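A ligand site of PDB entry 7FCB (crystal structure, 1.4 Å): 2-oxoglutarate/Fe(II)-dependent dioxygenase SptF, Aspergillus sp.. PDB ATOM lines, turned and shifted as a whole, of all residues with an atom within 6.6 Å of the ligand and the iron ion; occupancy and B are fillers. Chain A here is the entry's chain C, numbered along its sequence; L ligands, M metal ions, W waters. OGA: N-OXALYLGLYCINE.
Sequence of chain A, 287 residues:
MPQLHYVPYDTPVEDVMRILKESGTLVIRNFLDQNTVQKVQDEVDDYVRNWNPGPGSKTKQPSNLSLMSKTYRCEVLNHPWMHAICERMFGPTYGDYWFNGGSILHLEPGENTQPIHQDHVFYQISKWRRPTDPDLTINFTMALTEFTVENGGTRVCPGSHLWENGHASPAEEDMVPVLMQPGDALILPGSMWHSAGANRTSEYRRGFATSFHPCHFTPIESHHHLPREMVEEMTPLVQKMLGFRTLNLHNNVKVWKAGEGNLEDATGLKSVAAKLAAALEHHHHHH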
ATOM      1  N   THR A  59       8.417 -19.485  -6.022  1.00  0.00           N
ATOM      2  CA  THR A  59       9.586 -18.635  -5.849  1.00  0.00           C
ATOM      3  C   THR A  59       9.104 -17.195  -5.745  1.00  0.00           C
ATOM      4  O   THR A  59       8.310 -16.751  -6.577  1.00  0.00           O
ATOM      5  CB  THR A  59      10.560 -18.777  -7.025  1.00  0.00           C
ATOM      6  OG1 THR A  59      11.125 -20.094  -7.011  1.00  0.00           O
ATOM      7  CG2 THR A  59      11.693 -17.751  -6.921  1.00  0.00           C
ATOM      8  N   GLN A  61      10.753 -13.345  -5.556  1.00  0.00           N
ATOM      9  CA  GLN A  61      11.943 -12.493  -5.658  1.00  0.00           C
ATOM     10  C   GLN A  61      11.586 -11.017  -5.719  1.00  0.00           C
ATOM     11  O   GLN A  61      11.890 -10.330  -6.697  1.00  0.00           O
ATOM     12  CB  GLN A  61      12.795 -12.899  -6.854  1.00  0.00           C
ATOM     13  CG  GLN A  61      13.413 -14.287  -6.741  1.00  0.00           C
ATOM     14  CD  GLN A  61      14.613 -14.461  -7.638  1.00  0.00           C
ATOM     15  OE1 GLN A  61      15.069 -13.511  -8.286  1.00  0.00           O
ATOM     16  NE2 GLN A  61      15.132 -15.689  -7.701  1.00  0.00           N
ATOM     17  N   SER A 103      17.483  -8.688  -4.678  1.00  0.00           N
ATOM     18  CA  SER A 103      16.156  -9.133  -4.293  1.00  0.00           C
ATOM     19  C   SER A 103      16.220 -10.160  -3.186  1.00  0.00           C
ATOM     20  O   SER A 103      17.261 -10.741  -2.877  1.00  0.00           O
ATOM     21  CB  SER A 103      15.422  -9.730  -5.482  1.00  0.00           C
ATOM     22  OG  SER A 103      15.946 -10.995  -5.792  1.00  0.00           O
ATOM     23  N   LEU A 105      15.451 -13.839  -2.089  1.00  0.00           N
ATOM     24  CA  LEU A 105      15.540 -15.111  -2.802  1.00  0.00           C
ATOM     25  C   LEU A 105      14.812 -16.155  -1.953  1.00  0.00           C
ATOM     26  O   LEU A 105      15.413 -16.823  -1.115  1.00  0.00           O
ATOM     27  CB  LEU A 105      17.006 -15.488  -3.003  1.00  0.00           C
ATOM     28  CG  LEU A 105      17.835 -14.421  -3.714  1.00  0.00           C
ATOM     29  CD1 LEU A 105      19.311 -14.774  -3.600  1.00  0.00           C
ATOM     30  CD2 LEU A 105      17.443 -14.289  -5.186  1.00  0.00           C
ATOM     31  N   HIS A 106      13.521 -16.301  -2.196  1.00  0.00           N
ATOM     32  CA  HIS A 106      12.636 -17.057  -1.303  1.00  0.00           C
ATOM     33  C   HIS A 106      12.087 -18.272  -2.045  1.00  0.00           C
ATOM     34  O   HIS A 106      11.432 -18.122  -3.080  1.00  0.00           O
ATOM     35  CB  HIS A 106      11.494 -16.136  -0.865  1.00  0.00           C
ATOM     36  CG  HIS A 106      10.522 -16.782   0.069  1.00  0.00           C
ATOM     37  ND1 HIS A 106      10.569 -16.603   1.432  1.00  0.00           N
ATOM     38  CD2 HIS A 106       9.477 -17.613  -0.175  1.00  0.00           C
ATOM     39  CE1 HIS A 106       9.594 -17.294   1.990  1.00  0.00           C
ATOM     40  NE2 HIS A 106       8.917 -17.912   1.032  1.00  0.00           N
ATOM     41  N   LEU A 107      12.319 -19.460  -1.499  1.00  0.00           N
ATOM     42  CA  LEU A 107      11.815 -20.704  -2.068  1.00  0.00           C
ATOM     43  C   LEU A 107      10.766 -21.278  -1.130  1.00  0.00           C
ATOM     44  O   LEU A 107      11.081 -21.673   0.000  1.00  0.00           O
ATOM     45  CB  LEU A 107      12.924 -21.743  -2.225  1.00  0.00           C
ATOM     46  CG  LEU A 107      14.135 -21.378  -3.087  1.00  0.00           C
ATOM     47  CD1 LEU A 107      15.016 -22.600  -3.246  1.00  0.00           C
ATOM     48  CD2 LEU A 107      13.698 -20.800  -4.424  1.00  0.00           C
ATOM     49  N   GLN A 114      15.763 -24.463 -10.099  1.00  0.00           N
ATOM     50  CA  GLN A 114      15.852 -23.337 -11.004  1.00  0.00           C
ATOM     51  C   GLN A 114      16.795 -23.677 -12.158  1.00  0.00           C
ATOM     52  O   GLN A 114      17.773 -24.401 -11.959  1.00  0.00           O
ATOM     53  CB  GLN A 114      16.416 -22.137 -10.248  1.00  0.00           C
ATOM     54  CG  GLN A 114      16.554 -20.873 -11.071  1.00  0.00           C
ATOM     55  CD  GLN A 114      17.166 -19.758 -10.280  1.00  0.00           C
ATOM     56  OE1 GLN A 114      18.212 -19.915  -9.665  1.00  0.00           O
ATOM     57  NE2 GLN A 114      16.483 -18.627 -10.249  1.00  0.00           N
ATOM     58  N   HIS A 117      22.234 -21.190 -14.790  1.00  0.00           N
ATOM     59  CA  HIS A 117      22.413 -19.988 -15.611  1.00  0.00           C
ATOM     60  C   HIS A 117      23.662 -19.225 -15.163  1.00  0.00           C
ATOM     61  O   HIS A 117      24.195 -19.454 -14.076  1.00  0.00           O
ATOM     62  CB  HIS A 117      21.195 -19.062 -15.482  1.00  0.00           C
ATOM     63  CG  HIS A 117      20.953 -18.575 -14.091  1.00  0.00           C
ATOM     64  ND1 HIS A 117      20.316 -19.339 -13.126  1.00  0.00           N
ATOM     65  CD2 HIS A 117      21.321 -17.426 -13.470  1.00  0.00           C
ATOM     66  CE1 HIS A 117      20.273 -18.665 -11.990  1.00  0.00           C
ATOM     67  NE2 HIS A 117      20.870 -17.496 -12.179  1.00  0.00           N
ATOM     68  N   GLN A 118      24.108 -18.316 -16.033  1.00  0.00           N
ATOM     69  CA  GLN A 118      25.036 -17.259 -15.649  1.00  0.00           C
ATOM     70  C   GLN A 118      24.240 -15.971 -15.510  1.00  0.00           C
ATOM     71  O   GLN A 118      23.393 -15.665 -16.353  1.00  0.00           O
ATOM     72  CB  GLN A 118      26.084 -17.034 -16.733  1.00  0.00           C
ATOM     73  CG  GLN A 118      26.986 -18.235 -17.004  1.00  0.00           C
ATOM     74  CD  GLN A 118      27.886 -17.989 -18.195  1.00  0.00           C
ATOM     75  OE1 GLN A 118      27.388 -17.810 -19.316  1.00  0.00           O
ATOM     76  NE2 GLN A 118      29.192 -17.961 -17.970  1.00  0.00           N
ATOM     77  N   ASP A 119      24.513 -15.200 -14.439  1.00  0.00           N
ATOM     78  CA  ASP A 119      23.744 -13.970 -14.260  1.00  0.00           C
ATOM     79  C   ASP A 119      23.997 -12.946 -15.355  1.00  0.00           C
ATOM     80  O   ASP A 119      23.159 -12.078 -15.583  1.00  0.00           O
ATOM     81  CB  ASP A 119      24.050 -13.327 -12.900  1.00  0.00           C
ATOM     82  CG  ASP A 119      23.402 -14.049 -11.735  1.00  0.00           C
ATOM     83  OD1 ASP A 119      22.471 -14.868 -11.946  1.00  0.00           O
ATOM     84  OD2 ASP A 119      23.857 -13.769 -10.602  1.00  0.00           O
ATOM     85  N   ASN A 139      27.473 -10.653  -7.631  1.00  0.00           N
ATOM     86  CA  ASN A 139      26.332 -10.803  -6.732  1.00  0.00           C
ATOM     87  C   ASN A 139      26.832 -11.368  -5.397  1.00  0.00           C
ATOM     88  O   ASN A 139      27.764 -12.178  -5.373  1.00  0.00           O
ATOM     89  CB  ASN A 139      25.333 -11.762  -7.411  1.00  0.00           C
ATOM     90  CG  ASN A 139      24.295 -12.314  -6.468  1.00  0.00           C
ATOM     91  OD1 ASN A 139      24.606 -13.037  -5.547  1.00  0.00           O
ATOM     92  ND2 ASN A 139      23.026 -11.979  -6.729  1.00  0.00           N
ATOM     93  N   THR A 141      25.094 -13.319  -2.349  1.00  0.00           N
ATOM     94  CA  THR A 141      23.862 -14.020  -1.964  1.00  0.00           C
ATOM     95  C   THR A 141      24.004 -14.409  -0.490  1.00  0.00           C
ATOM     96  O   THR A 141      24.804 -15.300  -0.149  1.00  0.00           O
ATOM     97  CB  THR A 141      23.623 -15.212  -2.877  1.00  0.00           C
ATOM     98  OG1 THR A 141      23.151 -14.744  -4.146  1.00  0.00           O
ATOM     99  CG2 THR A 141      22.557 -16.161  -2.312  1.00  0.00           C
ATOM    100  N   PHE A 147      20.914 -22.607   4.392  1.00  0.00           N
ATOM    101  CA  PHE A 147      20.881 -23.165   3.044  1.00  0.00           C
ATOM    102  C   PHE A 147      21.387 -24.598   3.162  1.00  0.00           C
ATOM    103  O   PHE A 147      22.511 -24.825   3.624  1.00  0.00           O
ATOM    104  CB  PHE A 147      21.800 -22.388   2.109  1.00  0.00           C
ATOM    105  CG  PHE A 147      21.168 -21.165   1.465  1.00  0.00           C
ATOM    106  CD1 PHE A 147      20.206 -20.403   2.126  1.00  0.00           C
ATOM    107  CD2 PHE A 147      21.566 -20.767   0.192  1.00  0.00           C
ATOM    108  CE1 PHE A 147      19.673 -19.262   1.513  1.00  0.00           C
ATOM    109  CE2 PHE A 147      21.031 -19.655  -0.408  1.00  0.00           C
ATOM    110  CZ  PHE A 147      20.068 -18.899   0.241  1.00  0.00           C
ATOM    111  N   GLY A 152      16.964 -26.466  -1.019  1.00  0.00           N
ATOM    112  CA  GLY A 152      17.183 -25.744  -2.256  1.00  0.00           C
ATOM    113  C   GLY A 152      18.322 -24.746  -2.226  1.00  0.00           C
ATOM    114  O   GLY A 152      18.328 -23.827  -3.062  1.00  0.00           O
ATOM    115  N   GLY A 153      19.256 -24.882  -1.294  1.00  0.00           N
ATOM    116  CA  GLY A 153      20.432 -24.036  -1.275  1.00  0.00           C
ATOM    117  C   GLY A 153      21.063 -23.936  -2.647  1.00  0.00           C
ATOM    118  O   GLY A 153      21.101 -24.914  -3.412  1.00  0.00           O
ATOM    119  N   THR A 154      21.528 -22.732  -2.998  1.00  0.00           N
ATOM    120  CA  THR A 154      22.141 -22.484  -4.296  1.00  0.00           C
ATOM    121  C   THR A 154      23.229 -23.511  -4.581  1.00  0.00           C
ATOM    122  O   THR A 154      23.944 -23.968  -3.691  1.00  0.00           O
ATOM    123  CB  THR A 154      22.793 -21.090  -4.272  1.00  0.00           C
ATOM    124  OG1 THR A 154      21.905 -20.180  -3.605  1.00  0.00           O
ATOM    125  CG2 THR A 154      23.065 -20.593  -5.698  1.00  0.00           C
ATOM    126  N   ARG A 155      23.360 -23.869  -5.867  1.00  0.00           N
ATOM    127  CA  ARG A 155      24.409 -24.759  -6.328  1.00  0.00           C
ATOM    128  C   ARG A 155      25.263 -24.027  -7.355  1.00  0.00           C
ATOM    129  O   ARG A 155      24.760 -23.189  -8.113  1.00  0.00           O
ATOM    130  CB  ARG A 155      23.796 -26.004  -6.974  1.00  0.00           C
ATOM    131  CG  ARG A 155      22.757 -26.691  -6.102  1.00  0.00           C
ATOM    132  CD  ARG A 155      21.319 -26.255  -6.436  1.00  0.00           C
ATOM    133  NE  ARG A 155      21.092 -26.226  -7.872  1.00  0.00           N
ATOM    134  CZ  ARG A 155      20.965 -27.304  -8.627  1.00  0.00           C
ATOM    135  NH1 ARG A 155      20.942 -28.513  -8.094  1.00  0.00           N
ATOM    136  NH2 ARG A 155      20.887 -27.168  -9.951  1.00  0.00           N
ATOM    137  N   LEU A 186      27.426 -16.264  -0.224  1.00  0.00           N
ATOM    138  CA  LEU A 186      27.982 -16.836  -1.442  1.00  0.00           C
ATOM    139  C   LEU A 186      28.285 -15.726  -2.432  1.00  0.00           C
ATOM    140  O   LEU A 186      27.421 -14.877  -2.703  1.00  0.00           O
ATOM    141  CB  LEU A 186      26.955 -17.816  -2.017  1.00  0.00           C
ATOM    142  CG  LEU A 186      27.212 -18.425  -3.383  1.00  0.00           C
ATOM    143  CD1 LEU A 186      28.463 -19.306  -3.380  1.00  0.00           C
ATOM    144  CD2 LEU A 186      25.991 -19.223  -3.818  1.00  0.00           C
ATOM    145  N   LEU A 188      29.013 -14.597  -6.198  1.00  0.00           N
ATOM    146  CA  LEU A 188      28.659 -15.075  -7.536  1.00  0.00           C
ATOM    147  C   LEU A 188      29.033 -14.026  -8.565  1.00  0.00           C
ATOM    148  O   LEU A 188      28.225 -13.146  -8.886  1.00  0.00           O
ATOM    149  CB  LEU A 188      27.158 -15.368  -7.636  1.00  0.00           C
ATOM    150  CG  LEU A 188      26.661 -16.559  -6.837  1.00  0.00           C
ATOM    151  CD1 LEU A 188      25.147 -16.574  -6.875  1.00  0.00           C
ATOM    152  CD2 LEU A 188      27.241 -17.855  -7.401  1.00  0.00           C
ATOM    153  N   MET A 192      29.772 -17.130 -13.299  1.00  0.00           N
ATOM    154  CA  MET A 192      29.648 -18.438 -12.651  1.00  0.00           C
ATOM    155  C   MET A 192      28.296 -19.060 -12.962  1.00  0.00           C
ATOM    156  O   MET A 192      27.254 -18.433 -12.771  1.00  0.00           O
ATOM    157  CB  MET A 192      29.807 -18.274 -11.134  1.00  0.00           C
ATOM    158  CG  MET A 192      29.451 -19.532 -10.330  1.00  0.00           C
ATOM    159  SD  MET A 192      30.331 -21.024 -10.833  1.00  0.00           S
ATOM    160  CE  MET A 192      32.041 -20.559 -10.647  1.00  0.00           C
ATOM    161  N   HIS A 194      25.250 -21.322 -12.018  1.00  0.00           N
ATOM    162  CA  HIS A 194      24.666 -21.638 -10.723  1.00  0.00           C
ATOM    163  C   HIS A 194      23.146 -21.695 -10.851  1.00  0.00           C
ATOM    164  O   HIS A 194      22.563 -21.285 -11.860  1.00  0.00           O
ATOM    165  CB  HIS A 194      25.032 -20.555  -9.699  1.00  0.00           C
ATOM    166  CG  HIS A 194      24.458 -19.217 -10.040  1.00  0.00           C
ATOM    167  ND1 HIS A 194      25.020 -18.390 -10.990  1.00  0.00           N
ATOM    168  CD2 HIS A 194      23.344 -18.587  -9.597  1.00  0.00           C
ATOM    169  CE1 HIS A 194      24.285 -17.298 -11.101  1.00  0.00           C
ATOM    170  NE2 HIS A 194      23.254 -17.400 -10.284  1.00  0.00           N
ATOM    171  N   SER A 195      22.505 -22.163  -9.778  1.00  0.00           N
ATOM    172  CA  SER A 195      21.039 -22.105  -9.736  1.00  0.00           C
ATOM    173  C   SER A 195      20.556 -22.439  -8.331  1.00  0.00           C
ATOM    174  O   SER A 195      21.248 -23.106  -7.562  1.00  0.00           O
ATOM    175  CB  SER A 195      20.391 -23.073 -10.732  1.00  0.00           C
ATOM    176  OG  SER A 195      20.116 -24.330 -10.135  1.00  0.00           O
ATOM    177  N   ALA A 196      19.365 -21.938  -8.010  1.00  0.00           N
ATOM    178  CA  ALA A 196      18.662 -22.417  -6.828  1.00  0.00           C
ATOM    179  C   ALA A 196      18.273 -23.884  -7.023  1.00  0.00           C
ATOM    180  O   ALA A 196      17.995 -24.345  -8.133  1.00  0.00           O
ATOM    181  CB  ALA A 196      17.397 -21.575  -6.618  1.00  0.00           C
ATOM    182  N   GLY A 197      18.256 -24.625  -5.916  1.00  0.00           N
ATOM    183  CA  GLY A 197      17.814 -26.002  -5.939  1.00  0.00           C
ATOM    184  C   GLY A 197      16.338 -26.130  -5.625  1.00  0.00           C
ATOM    185  O   GLY A 197      15.623 -25.159  -5.395  1.00  0.00           O
ATOM    186  N   ARG A 205      13.033 -21.593   2.297  1.00  0.00           N
ATOM    187  CA  ARG A 205      14.447 -21.246   2.300  1.00  0.00           C
ATOM    188  C   ARG A 205      14.579 -19.822   1.771  1.00  0.00           C
ATOM    189  O   ARG A 205      14.107 -19.542   0.657  1.00  0.00           O
ATOM    190  CB  ARG A 205      15.249 -22.196   1.401  1.00  0.00           C
ATOM    191  CG  ARG A 205      16.740 -21.859   1.349  1.00  0.00           C
ATOM    192  CD  ARG A 205      17.271 -21.817  -0.083  1.00  0.00           C
ATOM    193  NE  ARG A 205      16.880 -20.586  -0.754  1.00  0.00           N
ATOM    194  CZ  ARG A 205      17.401 -20.175  -1.909  1.00  0.00           C
ATOM    195  NH1 ARG A 205      18.275 -20.923  -2.570  1.00  0.00           N
ATOM    196  NH2 ARG A 205      17.064 -18.987  -2.401  1.00  0.00           N
HETATM  197  C1  OGA L   1      18.847 -16.027  -9.425  1.00  0.00           C
HETATM  198  C2  OGA L   1      19.585 -17.046  -8.601  1.00  0.00           C
HETATM  199  C4  OGA L   1      19.756 -18.442  -6.634  1.00  0.00           C
HETATM  200  C5  OGA L   1      18.995 -18.835  -5.370  1.00  0.00           C
HETATM  201  O1  OGA L   1      17.659 -15.850  -9.145  1.00  0.00           O
HETATM  202  O2  OGA L   1      19.506 -15.463 -10.309  1.00  0.00           O
HETATM  203  O2' OGA L   1      20.697 -17.405  -8.981  1.00  0.00           O
HETATM  204  O3  OGA L   1      17.905 -18.273  -5.139  1.00  0.00           O
HETATM  205  N1  OGA L   1      19.042 -17.492  -7.468  1.00  0.00           N
HETATM  206  O4  OGA L   1      19.536 -19.688  -4.647  1.00  0.00           O
HETATM  207 FE    FE M   1      21.515 -16.214 -10.525  1.00  0.00          FE
HETATM  208  O   HOH W   1      18.022 -12.542  -8.234  1.00  0.00           O
HETATM  209  O   HOH W   2      18.798 -12.885 -10.947  1.00  0.00           O
HETATM  210  O   HOH W   3      21.592 -15.521  -6.294  1.00  0.00           O
HETATM  211  O   HOH W   4      15.476 -18.152  -6.623  1.00  0.00           O
HETATM  212  O   HOH W   5      22.052 -14.800  -8.985  1.00  0.00           O
HETATM  213  O   HOH W   6      15.885 -14.866 -11.243  1.00  0.00           O
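Residues that only touch the ligand: Leu 105 (3.6 Å) and Ala 196 (3.4 Å).
Hydrophobic or aromatic side chains within 4 Å of the ligand: Leu 105, His 117, His 194 and Ala 196.
Within 4 Å of the ligand: Gln 61, Leu 105, Gln 114, His 117, Asp 119, Thr 154, His 194, Ala 196 and Arg 205.
The nearest printed residue that does not touch the ligand is Ser 195 (4.4 Å).
An oxygen (O2') of the ligand is bound to the iron ion (2.1 Å).
A ring nitrogen (NE2) of His 194 is bound to the iron ion.
O2 of the ligand binds the iron ion (2.2 Å).
Water W5 binds the iron ion, 2.2 Å away.
The side-chain carboxylate (OD1) of Asp 119 binds the iron ion, at 2.2 Å.
NE2 of His 117 binds the iron ion (2.2 Å).
Water W4 bridges the side-chain amide nitrogen (NE2) of Gln 61 (2.7 Å) and an oxygen (O3) of the ligand (2.8 Å).
Water W6 bridges O1 of the ligand (2.9 Å) and OE1 of Gln 61 (3.4 Å).
Water W3 bridges OG1 of Thr 141 (2.8 Å) and N1 of the ligand (3.4 Å).
Water W1 bridges the side-chain amide oxygen (OE1) of Gln 61 (3.1 Å) and an oxygen (O1) of the ligand (3.5 Å).
Within 4 Å of the iron ion: His 117, Asp 119 and His 194.
The nearest printed residue that does not touch the iron ion is Gln 114 (5.0 Å).
The backbone NH of Leu 107 lies within hydrogen-bond range of the backbone carbonyl oxygen of Arg 205 (2.8 Å).
The backbone carbonyl oxygen (O) of Gln 114 sits at hydrogen-bond distance from the side-chain hydroxyl (OG) of Ser 195, at 3.0 Å.
A ring nitrogen (ND1) of His 194 lies within hydrogen-bond range of the backbone carbonyl oxygen of Met 192 (2.9 Å).
The guanidinium group (NH1) of Arg 205 lies within hydrogen-bond range of the backbone carbonyl oxygen (O) of Gly 152.
O of Leu 105 sits at hydrogen-bond distance from NH2 of Arg 205 (3.0 Å).
The side-chain amide oxygen (OE1) of Gln 114 sits at hydrogen-bond distance from the backbone NH (N) of Ala 196, 2.9 Å away.
NE2 of Gln 114 lies within hydrogen-bond range of O1 of the ligand (3.2 Å).
The guanidinium group (NH1) of Arg 205 lies within salt-bridge range of an oxygen (O4) of the ligand, at 2.7 Å.
An oxygen (O1) of the ligand is in hydrogen-bond range of the side-chain amide nitrogen (NE2) of Gln 61, 2.9 Å away.
An oxygen (O4) of the ligand lies within hydrogen-bond range of the side-chain hydroxyl (OG1) of Thr 154, 2.6 Å away.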
